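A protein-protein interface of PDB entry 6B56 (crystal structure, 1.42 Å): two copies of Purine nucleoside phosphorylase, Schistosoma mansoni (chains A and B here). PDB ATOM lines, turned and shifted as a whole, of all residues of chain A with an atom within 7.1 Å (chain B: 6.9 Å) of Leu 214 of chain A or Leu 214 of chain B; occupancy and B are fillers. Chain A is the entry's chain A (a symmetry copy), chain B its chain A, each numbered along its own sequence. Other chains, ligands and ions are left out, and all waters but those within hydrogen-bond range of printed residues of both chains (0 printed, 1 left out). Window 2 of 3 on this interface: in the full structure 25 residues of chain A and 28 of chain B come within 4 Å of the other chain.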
ATOM      1  N   ILE A 138     -22.075   1.883 -30.992  1.00  0.00           N
ATOM      2  CA  ILE A 138     -22.955   0.715 -31.188  1.00  0.00           C
ATOM      3  C   ILE A 138     -24.330   1.244 -31.598  1.00  0.00           C
ATOM      4  O   ILE A 138     -25.031   1.901 -30.800  1.00  0.00           O
ATOM      5  CB  ILE A 138     -23.011  -0.206 -29.952  1.00  0.00           C
ATOM      6  CG1 ILE A 138     -21.623  -0.799 -29.650  1.00  0.00           C
ATOM      7  CG2 ILE A 138     -24.076  -1.326 -30.146  1.00  0.00           C
ATOM      8  CD1 ILE A 138     -21.538  -1.594 -28.392  1.00  0.00           C
ATOM      9  N   PHE A 140     -27.805   0.574 -32.390  1.00  0.00           N
ATOM     10  CA  PHE A 140     -28.924  -0.375 -32.331  1.00  0.00           C
ATOM     11  C   PHE A 140     -29.920  -0.147 -33.469  1.00  0.00           C
ATOM     12  O   PHE A 140     -30.364  -1.149 -34.067  1.00  0.00           O
ATOM     13  CB  PHE A 140     -29.573  -0.411 -30.925  1.00  0.00           C
ATOM     14  CG  PHE A 140     -28.663  -0.975 -29.864  1.00  0.00           C
ATOM     15  CD1 PHE A 140     -28.524  -2.351 -29.748  1.00  0.00           C
ATOM     16  CD2 PHE A 140     -27.947  -0.151 -29.001  1.00  0.00           C
ATOM     17  CE1 PHE A 140     -27.675  -2.916 -28.792  1.00  0.00           C
ATOM     18  CE2 PHE A 140     -27.090  -0.724 -28.028  1.00  0.00           C
ATOM     19  CZ  PHE A 140     -26.959  -2.097 -27.946  1.00  0.00           C
ATOM     20  N   VAL A 193     -16.986   4.520 -25.975  1.00  0.00           N
ATOM     21  CA  VAL A 193     -17.906   4.004 -27.002  1.00  0.00           C
ATOM     22  C   VAL A 193     -19.337   4.465 -26.699  1.00  0.00           C
ATOM     23  O   VAL A 193     -19.813   4.299 -25.564  1.00  0.00           O
ATOM     24  CB  VAL A 193     -17.837   2.467 -27.037  1.00  0.00           C
ATOM     25  CG1 VAL A 193     -18.902   1.903 -27.994  1.00  0.00           C
ATOM     26  CG2 VAL A 193     -16.426   1.965 -27.436  1.00  0.00           C
ATOM     27  N   GLU A 207     -31.837  -2.051 -19.183  1.00  0.00           N
ATOM     28  CA  GLU A 207     -31.105  -1.734 -20.413  1.00  0.00           C
ATOM     29  C   GLU A 207     -29.714  -1.176 -20.094  1.00  0.00           C
ATOM     30  O   GLU A 207     -28.731  -1.525 -20.753  1.00  0.00           O
ATOM     31  CB  GLU A 207     -31.930  -0.768 -21.276  1.00  0.00           C
ATOM     32  CG  GLU A 207     -33.172  -1.406 -21.905  1.00  0.00           C
ATOM     33  CD  GLU A 207     -34.273  -0.419 -22.330  1.00  0.00           C
ATOM     34  OE1 GLU A 207     -34.063   0.821 -22.292  1.00  0.00           O
ATOM     35  OE2 GLU A 207     -35.375  -0.904 -22.698  1.00  0.00           O
ATOM     36  N   SER A 208     -29.607  -0.318 -19.066  1.00  0.00           N
ATOM     37  CA  SER A 208     -28.300   0.198 -18.659  1.00  0.00           C
ATOM     38  C   SER A 208     -27.359  -0.939 -18.265  1.00  0.00           C
ATOM     39  O   SER A 208     -26.193  -0.964 -18.689  1.00  0.00           O
ATOM     40  CB  SER A 208     -28.449   1.187 -17.492  1.00  0.00           C
ATOM     41  OG  SER A 208     -29.242   2.302 -17.868  1.00  0.00           O
ATOM     42  N   ASN A 209     -27.849  -1.895 -17.469  1.00  0.00           N
ATOM     43  CA  ASN A 209     -27.025  -3.048 -17.079  1.00  0.00           C
ATOM     44  C   ASN A 209     -26.583  -3.866 -18.293  1.00  0.00           C
ATOM     45  O   ASN A 209     -25.446  -4.364 -18.340  1.00  0.00           O
ATOM     46  CB  ASN A 209     -27.795  -3.941 -16.098  1.00  0.00           C
ATOM     47  CG  ASN A 209     -27.839  -3.373 -14.698  1.00  0.00           C
ATOM     48  OD1 ASN A 209     -26.961  -2.607 -14.296  1.00  0.00           O
ATOM     49  ND2 ASN A 209     -28.863  -3.754 -13.939  1.00  0.00           N
ATOM     50  N   MET A 210     -27.468  -4.028 -19.280  1.00  0.00           N
ATOM     51  CA  MET A 210     -27.095  -4.727 -20.512  1.00  0.00           C
ATOM     52  C   MET A 210     -25.971  -4.005 -21.251  1.00  0.00           C
ATOM     53  O   MET A 210     -25.009  -4.638 -21.720  1.00  0.00           O
ATOM     54  CB  MET A 210     -28.328  -4.911 -21.405  1.00  0.00           C
ATOM     55  CG  MET A 210     -28.000  -5.480 -22.766  1.00  0.00           C
ATOM     56  SD  MET A 210     -29.418  -5.680 -23.884  1.00  0.00           S
ATOM     57  CE  MET A 210     -29.632  -4.080 -24.486  1.00  0.00           C
ATOM     58  N   LEU A 211     -26.076  -2.672 -21.374  1.00  0.00           N
ATOM     59  CA  LEU A 211     -25.065  -1.881 -22.082  1.00  0.00           C
ATOM     60  C   LEU A 211     -23.707  -1.970 -21.403  1.00  0.00           C
ATOM     61  O   LEU A 211     -22.677  -1.971 -22.085  1.00  0.00           O
ATOM     62  CB  LEU A 211     -25.532  -0.424 -22.191  1.00  0.00           C
ATOM     63  CG  LEU A 211     -26.788  -0.196 -23.030  1.00  0.00           C
ATOM     64  CD1 LEU A 211     -27.165   1.288 -23.007  1.00  0.00           C
ATOM     65  CD2 LEU A 211     -26.630  -0.666 -24.478  1.00  0.00           C
ATOM     66  N   LEU A 212     -23.676  -2.072 -20.072  1.00  0.00           N
ATOM     67  CA  LEU A 212     -22.416  -2.301 -19.372  1.00  0.00           C
ATOM     68  C   LEU A 212     -21.791  -3.617 -19.815  1.00  0.00           C
ATOM     69  O   LEU A 212     -20.594  -3.673 -20.131  1.00  0.00           O
ATOM     70  CB  LEU A 212     -22.630  -2.270 -17.856  1.00  0.00           C
ATOM     71  CG  LEU A 212     -21.411  -2.456 -16.941  1.00  0.00           C
ATOM     72  CD1 LEU A 212     -20.418  -1.326 -17.074  1.00  0.00           C
ATOM     73  CD2 LEU A 212     -21.887  -2.567 -15.499  1.00  0.00           C
ATOM     74  N   LYS A 213     -22.595  -4.688 -19.850  1.00  0.00           N
ATOM     75  CA  LYS A 213     -22.078  -5.991 -20.288  1.00  0.00           C
ATOM     76  C   LYS A 213     -21.518  -5.935 -21.710  1.00  0.00           C
ATOM     77  O   LYS A 213     -20.607  -6.709 -22.041  1.00  0.00           O
ATOM     78  CB  LYS A 213     -23.182  -7.071 -20.207  1.00  0.00           C
ATOM     79  CG  LYS A 213     -23.735  -7.405 -18.815  1.00  0.00           C
ATOM     80  CD  LYS A 213     -24.892  -8.459 -18.887  1.00  0.00           C
ATOM     81  CE  LYS A 213     -25.295  -9.036 -17.534  1.00  0.00           C
ATOM     82  NZ  LYS A 213     -26.151  -8.132 -16.719  1.00  0.00           N
ATOM     83  N   LEU A 214     -22.083  -5.099 -22.582  1.00  0.00           N
ATOM     84  CA  LEU A 214     -21.742  -5.091 -24.010  1.00  0.00           C
ATOM     85  C   LEU A 214     -20.608  -4.142 -24.381  1.00  0.00           C
ATOM     86  O   LEU A 214     -20.324  -3.977 -25.576  1.00  0.00           O
ATOM     87  CB  LEU A 214     -22.966  -4.730 -24.840  1.00  0.00           C
ATOM     88  CG  LEU A 214     -24.094  -5.738 -24.753  1.00  0.00           C
ATOM     89  CD1 LEU A 214     -25.234  -5.281 -25.628  1.00  0.00           C
ATOM     90  CD2 LEU A 214     -23.575  -7.131 -25.151  1.00  0.00           C
ATOM     91  N   GLY A 215     -19.966  -3.524 -23.400  1.00  0.00           N
ATOM     92  CA  GLY A 215     -18.823  -2.673 -23.658  1.00  0.00           C
ATOM     93  C   GLY A 215     -19.124  -1.229 -24.000  1.00  0.00           C
ATOM     94  O   GLY A 215     -18.256  -0.533 -24.547  1.00  0.00           O
ATOM     95  N   CYS A 216     -20.304  -0.734 -23.660  1.00  0.00           N
ATOM     96  CA  CYS A 216     -20.634   0.660 -23.907  1.00  0.00           C
ATOM     97  C   CYS A 216     -20.187   1.527 -22.740  1.00  0.00           C
ATOM     98  O   CYS A 216     -20.285   1.130 -21.575  1.00  0.00           O
ATOM     99  CB  CYS A 216     -22.142   0.822 -24.099  1.00  0.00           C
ATOM    100  SG  CYS A 216     -22.861  -0.154 -25.450  1.00  0.00           S
ATOM    101  N   ASP A 217     -19.701   2.725 -23.061  1.00  0.00           N
ATOM    102  CA  ASP A 217     -19.305   3.694 -22.044  1.00  0.00           C
ATOM    103  C   ASP A 217     -20.364   4.756 -21.774  1.00  0.00           C
ATOM    104  O   ASP A 217     -20.494   5.197 -20.625  1.00  0.00           O
ATOM    105  CB  ASP A 217     -18.008   4.393 -22.462  1.00  0.00           C
ATOM    106  CG  ASP A 217     -16.821   3.435 -22.527  1.00  0.00           C
ATOM    107  OD1 ASP A 217     -16.335   3.028 -21.440  1.00  0.00           O
ATOM    108  OD2 ASP A 217     -16.369   3.085 -23.642  1.00  0.00           O
ATOM    109  N   ILE B 138     -29.104 -14.794 -35.258  1.00  0.00           N
ATOM    110  CA  ILE B 138     -29.551 -13.725 -34.347  1.00  0.00           C
ATOM    111  C   ILE B 138     -30.081 -12.581 -35.213  1.00  0.00           C
ATOM    112  O   ILE B 138     -29.316 -11.921 -35.948  1.00  0.00           O
ATOM    113  CB  ILE B 138     -28.449 -13.273 -33.367  1.00  0.00           C
ATOM    114  CG1 ILE B 138     -28.031 -14.432 -32.445  1.00  0.00           C
ATOM    115  CG2 ILE B 138     -28.914 -12.034 -32.545  1.00  0.00           C
ATOM    116  CD1 ILE B 138     -26.873 -14.142 -31.553  1.00  0.00           C
ATOM    117  N   PHE B 140     -31.412  -9.214 -35.436  1.00  0.00           N
ATOM    118  CA  PHE B 140     -31.616  -7.921 -34.772  1.00  0.00           C
ATOM    119  C   PHE B 140     -32.845  -7.193 -35.318  1.00  0.00           C
ATOM    120  O   PHE B 140     -33.609  -6.642 -34.498  1.00  0.00           O
ATOM    121  CB  PHE B 140     -30.326  -7.064 -34.774  1.00  0.00           C
ATOM    122  CG  PHE B 140     -29.222  -7.649 -33.930  1.00  0.00           C
ATOM    123  CD1 PHE B 140     -29.247  -7.465 -32.554  1.00  0.00           C
ATOM    124  CD2 PHE B 140     -28.180  -8.381 -34.492  1.00  0.00           C
ATOM    125  CE1 PHE B 140     -28.256  -8.007 -31.731  1.00  0.00           C
ATOM    126  CE2 PHE B 140     -27.172  -8.926 -33.658  1.00  0.00           C
ATOM    127  CZ  PHE B 140     -27.231  -8.741 -32.290  1.00  0.00           C
ATOM    128  N   VAL B 193     -23.168 -19.471 -36.223  1.00  0.00           N
ATOM    129  CA  VAL B 193     -24.363 -18.637 -36.020  1.00  0.00           C
ATOM    130  C   VAL B 193     -24.208 -17.310 -36.775  1.00  0.00           C
ATOM    131  O   VAL B 193     -23.175 -16.635 -36.632  1.00  0.00           O
ATOM    132  CB  VAL B 193     -24.566 -18.374 -34.517  1.00  0.00           C
ATOM    133  CG1 VAL B 193     -25.719 -17.377 -34.297  1.00  0.00           C
ATOM    134  CG2 VAL B 193     -24.824 -19.687 -33.735  1.00  0.00           C
ATOM    135  N   ASP B 206     -16.681  -1.589 -32.873  1.00  0.00           N
ATOM    136  CA  ASP B 206     -17.269  -1.870 -31.567  1.00  0.00           C
ATOM    137  C   ASP B 206     -18.511  -2.752 -31.657  1.00  0.00           C
ATOM    138  O   ASP B 206     -18.752  -3.565 -30.748  1.00  0.00           O
ATOM    139  CB  ASP B 206     -17.524  -0.573 -30.818  1.00  0.00           C
ATOM    140  CG  ASP B 206     -16.215   0.134 -30.487  1.00  0.00           C
ATOM    141  OD1 ASP B 206     -15.427  -0.406 -29.664  1.00  0.00           O
ATOM    142  OD2 ASP B 206     -15.910   1.175 -31.108  1.00  0.00           O
ATOM    143  N   ASN B 209     -17.021  -6.260 -31.841  1.00  0.00           N
ATOM    144  CA  ASN B 209     -16.658  -6.741 -30.501  1.00  0.00           C
ATOM    145  C   ASN B 209     -17.887  -7.181 -29.703  1.00  0.00           C
ATOM    146  O   ASN B 209     -17.834  -8.176 -28.960  1.00  0.00           O
ATOM    147  CB  ASN B 209     -15.901  -5.649 -29.734  1.00  0.00           C
ATOM    148  CG  ASN B 209     -14.464  -5.508 -30.181  1.00  0.00           C
ATOM    149  OD1 ASN B 209     -13.861  -6.456 -30.686  1.00  0.00           O
ATOM    150  ND2 ASN B 209     -13.901  -4.318 -29.989  1.00  0.00           N
ATOM    151  N   MET B 210     -18.997  -6.451 -29.833  1.00  0.00           N
ATOM    152  CA  MET B 210     -20.239  -6.854 -29.168  1.00  0.00           C
ATOM    153  C   MET B 210     -20.729  -8.211 -29.666  1.00  0.00           C
ATOM    154  O   MET B 210     -21.132  -9.074 -28.867  1.00  0.00           O
ATOM    155  CB  MET B 210     -21.307  -5.769 -29.350  1.00  0.00           C
ATOM    156  CG  MET B 210     -22.667  -6.178 -28.833  1.00  0.00           C
ATOM    157  SD  MET B 210     -23.984  -4.946 -29.059  1.00  0.00           S
ATOM    158  CE  MET B 210     -24.421  -5.185 -30.708  1.00  0.00           C
ATOM    159  N   LEU B 211     -20.711  -8.420 -30.993  1.00  0.00           N
ATOM    160  CA  LEU B 211     -21.178  -9.678 -31.582  1.00  0.00           C
ATOM    161  C   LEU B 211     -20.336 -10.858 -31.125  1.00  0.00           C
ATOM    162  O   LEU B 211     -20.865 -11.959 -30.940  1.00  0.00           O
ATOM    163  CB  LEU B 211     -21.181  -9.563 -33.111  1.00  0.00           C
ATOM    164  CG  LEU B 211     -22.152  -8.537 -33.692  1.00  0.00           C
ATOM    165  CD1 LEU B 211     -22.010  -8.494 -35.217  1.00  0.00           C
ATOM    166  CD2 LEU B 211     -23.609  -8.817 -33.318  1.00  0.00           C
ATOM    167  N   LEU B 212     -19.033 -10.654 -30.911  1.00  0.00           N
ATOM    168  CA  LEU B 212     -18.199 -11.707 -30.339  1.00  0.00           C
ATOM    169  C   LEU B 212     -18.701 -12.092 -28.954  1.00  0.00           C
ATOM    170  O   LEU B 212     -18.855 -13.283 -28.646  1.00  0.00           O
ATOM    171  CB  LEU B 212     -16.733 -11.266 -30.295  1.00  0.00           C
ATOM    172  CG  LEU B 212     -15.688 -12.253 -29.757  1.00  0.00           C
ATOM    173  CD1 LEU B 212     -15.553 -13.477 -30.632  1.00  0.00           C
ATOM    174  CD2 LEU B 212     -14.347 -11.542 -29.643  1.00  0.00           C
ATOM    175  N   LYS B 213     -18.969 -11.090 -28.105  1.00  0.00           N
ATOM    176  CA  LYS B 213     -19.480 -11.374 -26.758  1.00  0.00           C
ATOM    177  C   LYS B 213     -20.795 -12.152 -26.798  1.00  0.00           C
ATOM    178  O   LYS B 213     -21.086 -12.913 -25.863  1.00  0.00           O
ATOM    179  CB  LYS B 213     -19.675 -10.063 -25.962  1.00  0.00           C
ATOM    180  CG  LYS B 213     -18.419  -9.236 -25.653  1.00  0.00           C
ATOM    181  CD  LYS B 213     -18.770  -7.904 -24.907  1.00  0.00           C
ATOM    182  CE  LYS B 213     -17.560  -7.175 -24.332  1.00  0.00           C
ATOM    183  NZ  LYS B 213     -16.771  -6.418 -25.341  1.00  0.00           N
ATOM    184  N   LEU B 214     -21.635 -11.928 -27.810  1.00  0.00           N
ATOM    185  CA  LEU B 214     -22.992 -12.486 -27.855  1.00  0.00           C
ATOM    186  C   LEU B 214     -23.093 -13.843 -28.540  1.00  0.00           C
ATOM    187  O   LEU B 214     -24.211 -14.343 -28.732  1.00  0.00           O
ATOM    188  CB  LEU B 214     -23.934 -11.518 -28.557  1.00  0.00           C
ATOM    189  CG  LEU B 214     -24.119 -10.198 -27.835  1.00  0.00           C
ATOM    190  CD1 LEU B 214     -25.083  -9.339 -28.615  1.00  0.00           C
ATOM    191  CD2 LEU B 214     -24.600 -10.458 -26.397  1.00  0.00           C
ATOM    192  N   GLY B 215     -21.969 -14.440 -28.911  1.00  0.00           N
ATOM    193  CA  GLY B 215     -21.969 -15.767 -29.490  1.00  0.00           C
ATOM    194  C   GLY B 215     -22.180 -15.846 -30.988  1.00  0.00           C
ATOM    195  O   GLY B 215     -22.519 -16.921 -31.505  1.00  0.00           O
ATOM    196  N   CYS B 216     -21.950 -14.764 -31.714  1.00  0.00           N
ATOM    197  CA  CYS B 216     -22.076 -14.789 -33.162  1.00  0.00           C
ATOM    198  C   CYS B 216     -20.767 -15.223 -33.804  1.00  0.00           C
ATOM    199  O   CYS B 216     -19.681 -14.856 -33.347  1.00  0.00           O
ATOM    200  CB  CYS B 216     -22.452 -13.403 -33.685  1.00  0.00           C
ATOM    201  SG  CYS B 216     -23.992 -12.713 -33.017  1.00  0.00           S
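Met 210 of chain B touches Ile 138 of chain A (SD to CG2, 3.8 Å).
Asp 206 of chain B touches Val 193 of chain A (OD1 to CG2, 3.4 Å).
Lys 213 of chain A touches Lys 213 of chain B (O to CD, 3.6 Å).
CD1 of Leu 214 of chain A touches SD of Met 210 of chain B (3.7 Å).
CD2 of Leu 214 of chain A touches CD2 of Leu 214 of chain B, 3.7 Å away.
Ile 138 of chain A touches Met 210 of chain B, but with the chains exchanged Met 210 of chain A does not touch Ile 138 of chain B (10.8 Å).
Lys 213 of chain A touches its own counterpart, Lys 213 of chain B.
Leu 214 of chain A touches Met 210 of chain B, but with the chains exchanged Met 210 of chain A does not touch Leu 214 of chain B (7.0 Å).
Leu 214 of chain B touches its own counterpart, Leu 214 of chain A.
Positions printed for both chains: 138, 140, 193, 209, 210, 211, 212, 213, 214, 215 and 216.
Of the 5 pairs that touch across the chains among the printed residues, 2 have their exchanged pair printed and touching as well.
N of Val 193 of chain A sits at hydrogen-bond distance from OD2 of Asp 217 of chain A, 2.8 Å away.
Of chain B, only Met 210 (3.7 Å) and Leu 214 (3.7 Å) come within 4 Å of Leu 214 of chain A.
Leu 214 of chain B touches just one residue of chain A: Leu 214.
Of the printed residues of chain A, Met 210 of chain B touches Ile 138 (3.8 Å) and Leu 214 (3.7 Å).
Printed residues of chain B within 4 Å of Val 193 of chain A: Asp 206.
Printed residues of chain B within 4 Å of Ile 138 of chain A: Met 210 (3.8 Å).
Of the printed residues of chain A, Lys 213 of chain B touches Lys 213 (3.6 Å).
Printed residues of chain A within 4 Å of Asp 206 of chain B: Val 193 (3.4 Å).
The nearest residue of chain A that does not touch Leu 214 of chain B is Phe 140 of chain A (6.9 Å).
Hydrophobic or aromatic side chains of chain B within 4 Å of the printed part of chain A: Met 210 and Leu 214.
Hydrophobic or aromatic side chains of chain A that line the printed part of chain B: Ile 138, Val 193 and Leu 214.
Among the printed residues, no Asp or Glu carboxylate lies within 4 Å of a Lys or Arg side-chain nitrogen of the other chain.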
